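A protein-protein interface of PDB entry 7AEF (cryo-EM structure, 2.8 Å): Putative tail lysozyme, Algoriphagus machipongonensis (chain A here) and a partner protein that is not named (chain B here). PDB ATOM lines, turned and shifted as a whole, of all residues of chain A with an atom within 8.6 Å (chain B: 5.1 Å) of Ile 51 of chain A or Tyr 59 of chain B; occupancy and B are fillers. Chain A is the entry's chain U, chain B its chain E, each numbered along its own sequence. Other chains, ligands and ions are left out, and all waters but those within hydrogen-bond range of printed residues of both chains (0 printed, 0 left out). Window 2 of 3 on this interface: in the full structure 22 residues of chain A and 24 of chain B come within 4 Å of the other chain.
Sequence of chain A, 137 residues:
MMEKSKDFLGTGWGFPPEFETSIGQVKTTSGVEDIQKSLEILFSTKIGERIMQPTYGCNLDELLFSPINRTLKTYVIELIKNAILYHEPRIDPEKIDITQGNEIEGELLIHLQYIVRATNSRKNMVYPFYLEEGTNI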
ATOM      1  N   LYS A  46      26.676 -12.939  -1.509  1.00  0.00           N
ATOM      2  CA  LYS A  46      25.943 -11.750  -1.916  1.00  0.00           C
ATOM      3  C   LYS A  46      24.855 -12.100  -2.925  1.00  0.00           C
ATOM      4  O   LYS A  46      24.923 -13.121  -3.599  1.00  0.00           O
ATOM      5  CB  LYS A  46      26.915 -10.739  -2.510  1.00  0.00           C
ATOM      6  CG  LYS A  46      27.973 -10.314  -1.528  1.00  0.00           C
ATOM      7  CD  LYS A  46      28.950  -9.378  -2.172  1.00  0.00           C
ATOM      8  CE  LYS A  46      30.139  -9.077  -1.284  1.00  0.00           C
ATOM      9  NZ  LYS A  46      29.778  -8.427  -0.028  1.00  0.00           N
ATOM     10  N   ILE A  47      23.868 -11.208  -3.051  1.00  0.00           N
ATOM     11  CA  ILE A  47      22.644 -11.501  -3.808  1.00  0.00           C
ATOM     12  C   ILE A  47      22.906 -11.860  -5.278  1.00  0.00           C
ATOM     13  O   ILE A  47      22.318 -12.814  -5.804  1.00  0.00           O
ATOM     14  CB  ILE A  47      21.679 -10.313  -3.705  1.00  0.00           C
ATOM     15  CG1 ILE A  47      21.187 -10.140  -2.268  1.00  0.00           C
ATOM     16  CG2 ILE A  47      20.509 -10.473  -4.657  1.00  0.00           C
ATOM     17  CD1 ILE A  47      20.317 -11.239  -1.745  1.00  0.00           C
ATOM     18  N   GLY A  48      23.774 -11.126  -5.962  1.00  0.00           N
ATOM     19  CA  GLY A  48      24.000 -11.401  -7.370  1.00  0.00           C
ATOM     20  C   GLY A  48      25.143 -12.338  -7.723  1.00  0.00           C
ATOM     21  O   GLY A  48      25.509 -12.414  -8.898  1.00  0.00           O
ATOM     22  N   GLU A  49      25.727 -13.064  -6.763  1.00  0.00           N
ATOM     23  CA  GLU A  49      26.910 -13.882  -7.050  1.00  0.00           C
ATOM     24  C   GLU A  49      26.643 -15.231  -7.723  1.00  0.00           C
ATOM     25  O   GLU A  49      27.577 -15.794  -8.297  1.00  0.00           O
ATOM     26  CB  GLU A  49      27.711 -14.132  -5.777  1.00  0.00           C
ATOM     27  CG  GLU A  49      28.517 -12.926  -5.369  1.00  0.00           C
ATOM     28  CD  GLU A  49      29.298 -13.110  -4.089  1.00  0.00           C
ATOM     29  OE1 GLU A  49      28.914 -13.922  -3.232  1.00  0.00           O
ATOM     30  OE2 GLU A  49      30.304 -12.413  -3.929  1.00  0.00           O
ATOM     31  N   ARG A  50      25.450 -15.797  -7.646  1.00  0.00           N
ATOM     32  CA  ARG A  50      25.214 -17.072  -8.305  1.00  0.00           C
ATOM     33  C   ARG A  50      24.760 -16.804  -9.742  1.00  0.00           C
ATOM     34  O   ARG A  50      24.099 -15.804 -10.000  1.00  0.00           O
ATOM     35  CB  ARG A  50      24.166 -17.874  -7.530  1.00  0.00           C
ATOM     36  CG  ARG A  50      24.520 -18.179  -6.078  1.00  0.00           C
ATOM     37  CD  ARG A  50      25.613 -19.200  -5.942  1.00  0.00           C
ATOM     38  NE  ARG A  50      25.236 -20.469  -6.552  1.00  0.00           N
ATOM     39  CZ  ARG A  50      24.521 -21.428  -5.965  1.00  0.00           C
ATOM     40  NH1 ARG A  50      24.090 -21.298  -4.724  1.00  0.00           N
ATOM     41  NH2 ARG A  50      24.233 -22.532  -6.628  1.00  0.00           N
ATOM     42  N   ILE A  51      25.087 -17.705 -10.677  1.00  0.00           N
ATOM     43  CA  ILE A  51      24.892 -17.395 -12.106  1.00  0.00           C
ATOM     44  C   ILE A  51      23.419 -17.452 -12.540  1.00  0.00           C
ATOM     45  O   ILE A  51      22.915 -16.514 -13.164  1.00  0.00           O
ATOM     46  CB  ILE A  51      25.751 -18.302 -12.997  1.00  0.00           C
ATOM     47  CG1 ILE A  51      27.246 -18.091 -12.719  1.00  0.00           C
ATOM     48  CG2 ILE A  51      25.440 -18.037 -14.476  1.00  0.00           C
ATOM     49  CD1 ILE A  51      27.789 -16.681 -12.941  1.00  0.00           C
ATOM     50  N   MET A  52      22.726 -18.561 -12.351  1.00  0.00           N
ATOM     51  CA  MET A  52      21.342 -18.506 -12.815  1.00  0.00           C
ATOM     52  C   MET A  52      20.372 -18.382 -11.662  1.00  0.00           C
ATOM     53  O   MET A  52      19.167 -18.564 -11.840  1.00  0.00           O
ATOM     54  CB  MET A  52      21.015 -19.673 -13.742  1.00  0.00           C
ATOM     55  CG  MET A  52      21.855 -19.664 -15.019  1.00  0.00           C
ATOM     56  SD  MET A  52      21.488 -18.399 -16.253  1.00  0.00           S
ATOM     57  CE  MET A  52      19.957 -18.955 -16.981  1.00  0.00           C
ATOM     58  N   GLN A  53      20.907 -18.037 -10.489  1.00  0.00           N
ATOM     59  CA  GLN A  53      20.180 -17.797  -9.247  1.00  0.00           C
ATOM     60  C   GLN A  53      20.453 -16.372  -8.773  1.00  0.00           C
ATOM     61  O   GLN A  53      21.096 -16.174  -7.735  1.00  0.00           O
ATOM     62  CB  GLN A  53      20.620 -18.798  -8.183  1.00  0.00           C
ATOM     63  CG  GLN A  53      20.366 -20.236  -8.510  1.00  0.00           C
ATOM     64  CD  GLN A  53      18.913 -20.572  -8.434  1.00  0.00           C
ATOM     65  OE1 GLN A  53      18.146 -19.900  -7.749  1.00  0.00           O
ATOM     66  NE2 GLN A  53      18.519 -21.619  -9.134  1.00  0.00           N
ATOM     67  N   PRO A  54      19.935 -15.368  -9.500  1.00  0.00           N
ATOM     68  CA  PRO A  54      20.243 -13.942  -9.265  1.00  0.00           C
ATOM     69  C   PRO A  54      19.752 -13.379  -7.947  1.00  0.00           C
ATOM     70  O   PRO A  54      20.059 -12.224  -7.627  1.00  0.00           O
ATOM     71  CB  PRO A  54      19.503 -13.262 -10.428  1.00  0.00           C
ATOM     72  CG  PRO A  54      18.426 -14.226 -10.799  1.00  0.00           C
ATOM     73  CD  PRO A  54      18.982 -15.533 -10.604  1.00  0.00           C
ATOM     74  N   THR A  55      18.938 -14.117  -7.210  1.00  0.00           N
ATOM     75  CA  THR A  55      18.420 -13.658  -5.934  1.00  0.00           C
ATOM     76  C   THR A  55      18.718 -14.700  -4.866  1.00  0.00           C
ATOM     77  O   THR A  55      17.786 -15.306  -4.352  1.00  0.00           O
ATOM     78  CB  THR A  55      16.916 -13.478  -6.013  1.00  0.00           C
ATOM     79  OG1 THR A  55      16.330 -14.746  -6.343  1.00  0.00           O
ATOM     80  CG2 THR A  55      16.538 -12.473  -7.057  1.00  0.00           C
ATOM     81  N   TYR A  56      19.973 -14.831  -4.452  1.00  0.00           N
ATOM     82  CA  TYR A  56      20.347 -15.820  -3.442  1.00  0.00           C
ATOM     83  C   TYR A  56      21.442 -15.233  -2.572  1.00  0.00           C
ATOM     84  O   TYR A  56      22.522 -14.942  -3.077  1.00  0.00           O
ATOM     85  CB  TYR A  56      20.840 -17.134  -4.075  1.00  0.00           C
ATOM     86  CG  TYR A  56      21.262 -18.140  -3.032  1.00  0.00           C
ATOM     87  CD1 TYR A  56      20.329 -18.961  -2.451  1.00  0.00           C
ATOM     88  CD2 TYR A  56      22.583 -18.251  -2.612  1.00  0.00           C
ATOM     89  CE1 TYR A  56      20.682 -19.849  -1.482  1.00  0.00           C
ATOM     90  CE2 TYR A  56      22.937 -19.124  -1.636  1.00  0.00           C
ATOM     91  CZ  TYR A  56      21.984 -19.924  -1.076  1.00  0.00           C
ATOM     92  OH  TYR A  56      22.341 -20.811  -0.104  1.00  0.00           O
ATOM     93  N   PHE B  22      20.029 -24.136 -21.094  1.00  0.00           N
ATOM     94  CA  PHE B  22      20.537 -24.287 -19.732  1.00  0.00           C
ATOM     95  C   PHE B  22      19.633 -25.137 -18.860  1.00  0.00           C
ATOM     96  O   PHE B  22      20.112 -26.009 -18.129  1.00  0.00           O
ATOM     97  CB  PHE B  22      20.707 -22.936 -19.054  1.00  0.00           C
ATOM     98  CG  PHE B  22      21.170 -23.050 -17.635  1.00  0.00           C
ATOM     99  CD1 PHE B  22      22.507 -23.198 -17.344  1.00  0.00           C
ATOM    100  CD2 PHE B  22      20.270 -23.021 -16.582  1.00  0.00           C
ATOM    101  CE1 PHE B  22      22.930 -23.316 -16.041  1.00  0.00           C
ATOM    102  CE2 PHE B  22      20.688 -23.155 -15.301  1.00  0.00           C
ATOM    103  CZ  PHE B  22      22.017 -23.295 -15.025  1.00  0.00           C
ATOM    104  N   GLU B  55      25.750 -26.542 -11.866  1.00  0.00           N
ATOM    105  CA  GLU B  55      25.261 -25.375 -12.580  1.00  0.00           C
ATOM    106  C   GLU B  55      26.382 -24.636 -13.302  1.00  0.00           C
ATOM    107  O   GLU B  55      26.191 -24.184 -14.434  1.00  0.00           O
ATOM    108  CB  GLU B  55      24.534 -24.446 -11.623  1.00  0.00           C
ATOM    109  CG  GLU B  55      23.207 -25.006 -11.145  1.00  0.00           C
ATOM    110  CD  GLU B  55      22.523 -24.106 -10.170  1.00  0.00           C
ATOM    111  OE1 GLU B  55      23.139 -23.130  -9.761  1.00  0.00           O
ATOM    112  OE2 GLU B  55      21.374 -24.367  -9.815  1.00  0.00           O
ATOM    113  N   VAL B  56      27.566 -24.554 -12.689  1.00  0.00           N
ATOM    114  CA  VAL B  56      28.703 -23.909 -13.341  1.00  0.00           C
ATOM    115  C   VAL B  56      29.089 -24.648 -14.606  1.00  0.00           C
ATOM    116  O   VAL B  56      29.347 -24.033 -15.647  1.00  0.00           O
ATOM    117  CB  VAL B  56      29.908 -23.823 -12.394  1.00  0.00           C
ATOM    118  CG1 VAL B  56      31.144 -23.365 -13.150  1.00  0.00           C
ATOM    119  CG2 VAL B  56      29.619 -22.858 -11.286  1.00  0.00           C
ATOM    120  N   LEU B  57      29.139 -25.971 -14.533  1.00  0.00           N
ATOM    121  CA  LEU B  57      29.491 -26.758 -15.701  1.00  0.00           C
ATOM    122  C   LEU B  57      28.461 -26.619 -16.810  1.00  0.00           C
ATOM    123  O   LEU B  57      28.835 -26.528 -17.980  1.00  0.00           O
ATOM    124  CB  LEU B  57      29.663 -28.213 -15.302  1.00  0.00           C
ATOM    125  CG  LEU B  57      30.857 -28.510 -14.390  1.00  0.00           C
ATOM    126  CD1 LEU B  57      30.749 -29.917 -13.912  1.00  0.00           C
ATOM    127  CD2 LEU B  57      32.176 -28.303 -15.105  1.00  0.00           C
ATOM    128  N   CYS B  58      27.171 -26.567 -16.469  1.00  0.00           N
ATOM    129  CA  CYS B  58      26.141 -26.421 -17.496  1.00  0.00           C
ATOM    130  C   CYS B  58      26.312 -25.120 -18.261  1.00  0.00           C
ATOM    131  O   CYS B  58      26.168 -25.082 -19.487  1.00  0.00           O
ATOM    132  CB  CYS B  58      24.756 -26.459 -16.868  1.00  0.00           C
ATOM    133  SG  CYS B  58      24.280 -28.045 -16.213  1.00  0.00           S
ATOM    134  N   TYR B  59      26.659 -24.059 -17.540  1.00  0.00           N
ATOM    135  CA  TYR B  59      26.917 -22.761 -18.139  1.00  0.00           C
ATOM    136  C   TYR B  59      28.083 -22.836 -19.122  1.00  0.00           C
ATOM    137  O   TYR B  59      27.986 -22.347 -20.250  1.00  0.00           O
ATOM    138  CB  TYR B  59      27.151 -21.776 -17.001  1.00  0.00           C
ATOM    139  CG  TYR B  59      27.442 -20.377 -17.347  1.00  0.00           C
ATOM    140  CD1 TYR B  59      26.481 -19.581 -17.915  1.00  0.00           C
ATOM    141  CD2 TYR B  59      28.657 -19.830 -17.036  1.00  0.00           C
ATOM    142  CE1 TYR B  59      26.732 -18.281 -18.190  1.00  0.00           C
ATOM    143  CE2 TYR B  59      28.912 -18.529 -17.301  1.00  0.00           C
ATOM    144  CZ  TYR B  59      27.950 -17.757 -17.879  1.00  0.00           C
ATOM    145  OH  TYR B  59      28.207 -16.442 -18.147  1.00  0.00           O
ATOM    146  N   ALA B  60      29.175 -23.489 -18.714  1.00  0.00           N
ATOM    147  CA  ALA B  60      30.342 -23.673 -19.575  1.00  0.00           C
ATOM    148  C   ALA B  60      30.017 -24.451 -20.847  1.00  0.00           C
ATOM    149  O   ALA B  60      30.552 -24.143 -21.917  1.00  0.00           O
ATOM    150  CB  ALA B  60      31.432 -24.391 -18.805  1.00  0.00           C
ATOM    151  N   ILE B  61      29.137 -25.450 -20.752  1.00  0.00           N
ATOM    152  CA  ILE B  61      28.752 -26.216 -21.933  1.00  0.00           C
ATOM    153  C   ILE B  61      28.048 -25.343 -22.949  1.00  0.00           C
ATOM    154  O   ILE B  61      28.333 -25.440 -24.145  1.00  0.00           O
ATOM    155  CB  ILE B  61      27.873 -27.417 -21.570  1.00  0.00           C
ATOM    156  CG1 ILE B  61      28.723 -28.429 -20.832  1.00  0.00           C
ATOM    157  CG2 ILE B  61      27.235 -28.028 -22.838  1.00  0.00           C
ATOM    158  CD1 ILE B  61      27.942 -29.520 -20.162  1.00  0.00           C
ATOM    159  N   SER B  62      27.124 -24.490 -22.499  1.00  0.00           N
ATOM    160  CA  SER B  62      26.424 -23.599 -23.417  1.00  0.00           C
ATOM    161  C   SER B  62      27.394 -22.730 -24.198  1.00  0.00           C
ATOM    162  O   SER B  62      27.217 -22.533 -25.402  1.00  0.00           O
ATOM    163  CB  SER B  62      25.470 -22.696 -22.664  1.00  0.00           C
ATOM    164  OG  SER B  62      24.448 -23.422 -22.046  1.00  0.00           O
ATOM    165  N   ASP B  63      28.442 -22.236 -23.530  1.00  0.00           N
ATOM    166  CA  ASP B  63      29.461 -21.422 -24.188  1.00  0.00           C
ATOM    167  C   ASP B  63      30.146 -22.191 -25.305  1.00  0.00           C
ATOM    168  O   ASP B  63      30.321 -21.669 -26.411  1.00  0.00           O
ATOM    169  CB  ASP B  63      30.487 -20.946 -23.157  1.00  0.00           C
ATOM    170  CG  ASP B  63      31.558 -20.031 -23.725  1.00  0.00           C
ATOM    171  OD1 ASP B  63      31.234 -19.100 -24.441  1.00  0.00           O
ATOM    172  OD2 ASP B  63      32.726 -20.213 -23.393  1.00  0.00           O
ATOM    173  N   GLU B 395      33.881 -18.754 -11.776  1.00  0.00           N
ATOM    174  CA  GLU B 395      32.441 -18.705 -11.664  1.00  0.00           C
ATOM    175  C   GLU B 395      31.950 -18.968 -10.248  1.00  0.00           C
ATOM    176  O   GLU B 395      30.742 -18.946 -10.014  1.00  0.00           O
ATOM    177  CB  GLU B 395      31.818 -19.735 -12.601  1.00  0.00           C
ATOM    178  CG  GLU B 395      32.151 -19.576 -14.072  1.00  0.00           C
ATOM    179  CD  GLU B 395      31.592 -18.349 -14.660  1.00  0.00           C
ATOM    180  OE1 GLU B 395      30.523 -17.945 -14.237  1.00  0.00           O
ATOM    181  OE2 GLU B 395      32.202 -17.790 -15.557  1.00  0.00           O
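Hydrophobic or aromatic side chains of chain B within 4 Å of the printed part of chain A: Phe 22 and Tyr 59.
Among the printed residues, 4 pairs touch across the chains.
Printed residues of chain B within 4 Å of Arg 50 of chain A: Glu 55.
Ile 51 of chain A touches just these residues of chain B: Tyr 59 (3.9 Å) and Glu 395 (3.3 Å).
Of the printed residues of chain B, Met 52 of chain A touches Phe 22.
Printed residues of chain A within 4 Å of Phe 22 of chain B: Met 52.
Printed residues of chain A within 4 Å of Glu 55 of chain B: Arg 50 (3.4 Å).
Of chain A, only Ile 51 comes within 4 Å of Tyr 59 of chain B.
No residue of chain A comes within 4 Å of Ala 60 of chain B.
Of the printed residues of chain A, Glu 395 of chain B touches Ile 51.
The nearest printed residue of chain B that does not touch Ile 51 of chain A is Val 56 of chain B (5.5 Å).
The nearest printed residue of chain B that does not touch Met 52 of chain A is Glu 55 of chain B (5.3 Å).
Among the printed residues, pairs that only touch across the chains: Ile 51 of chain A with Tyr 59 of chain B (3.9 Å), Ile 51 of chain A with Glu 395 of chain B (3.3 Å) and Met 52 of chain A with Phe 22 of chain B (3.6 Å).
The guanidinium group of Arg 50 of chain A lies within salt-bridge range of the side-chain carboxylate of Glu 55 of chain B (3.4 Å).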
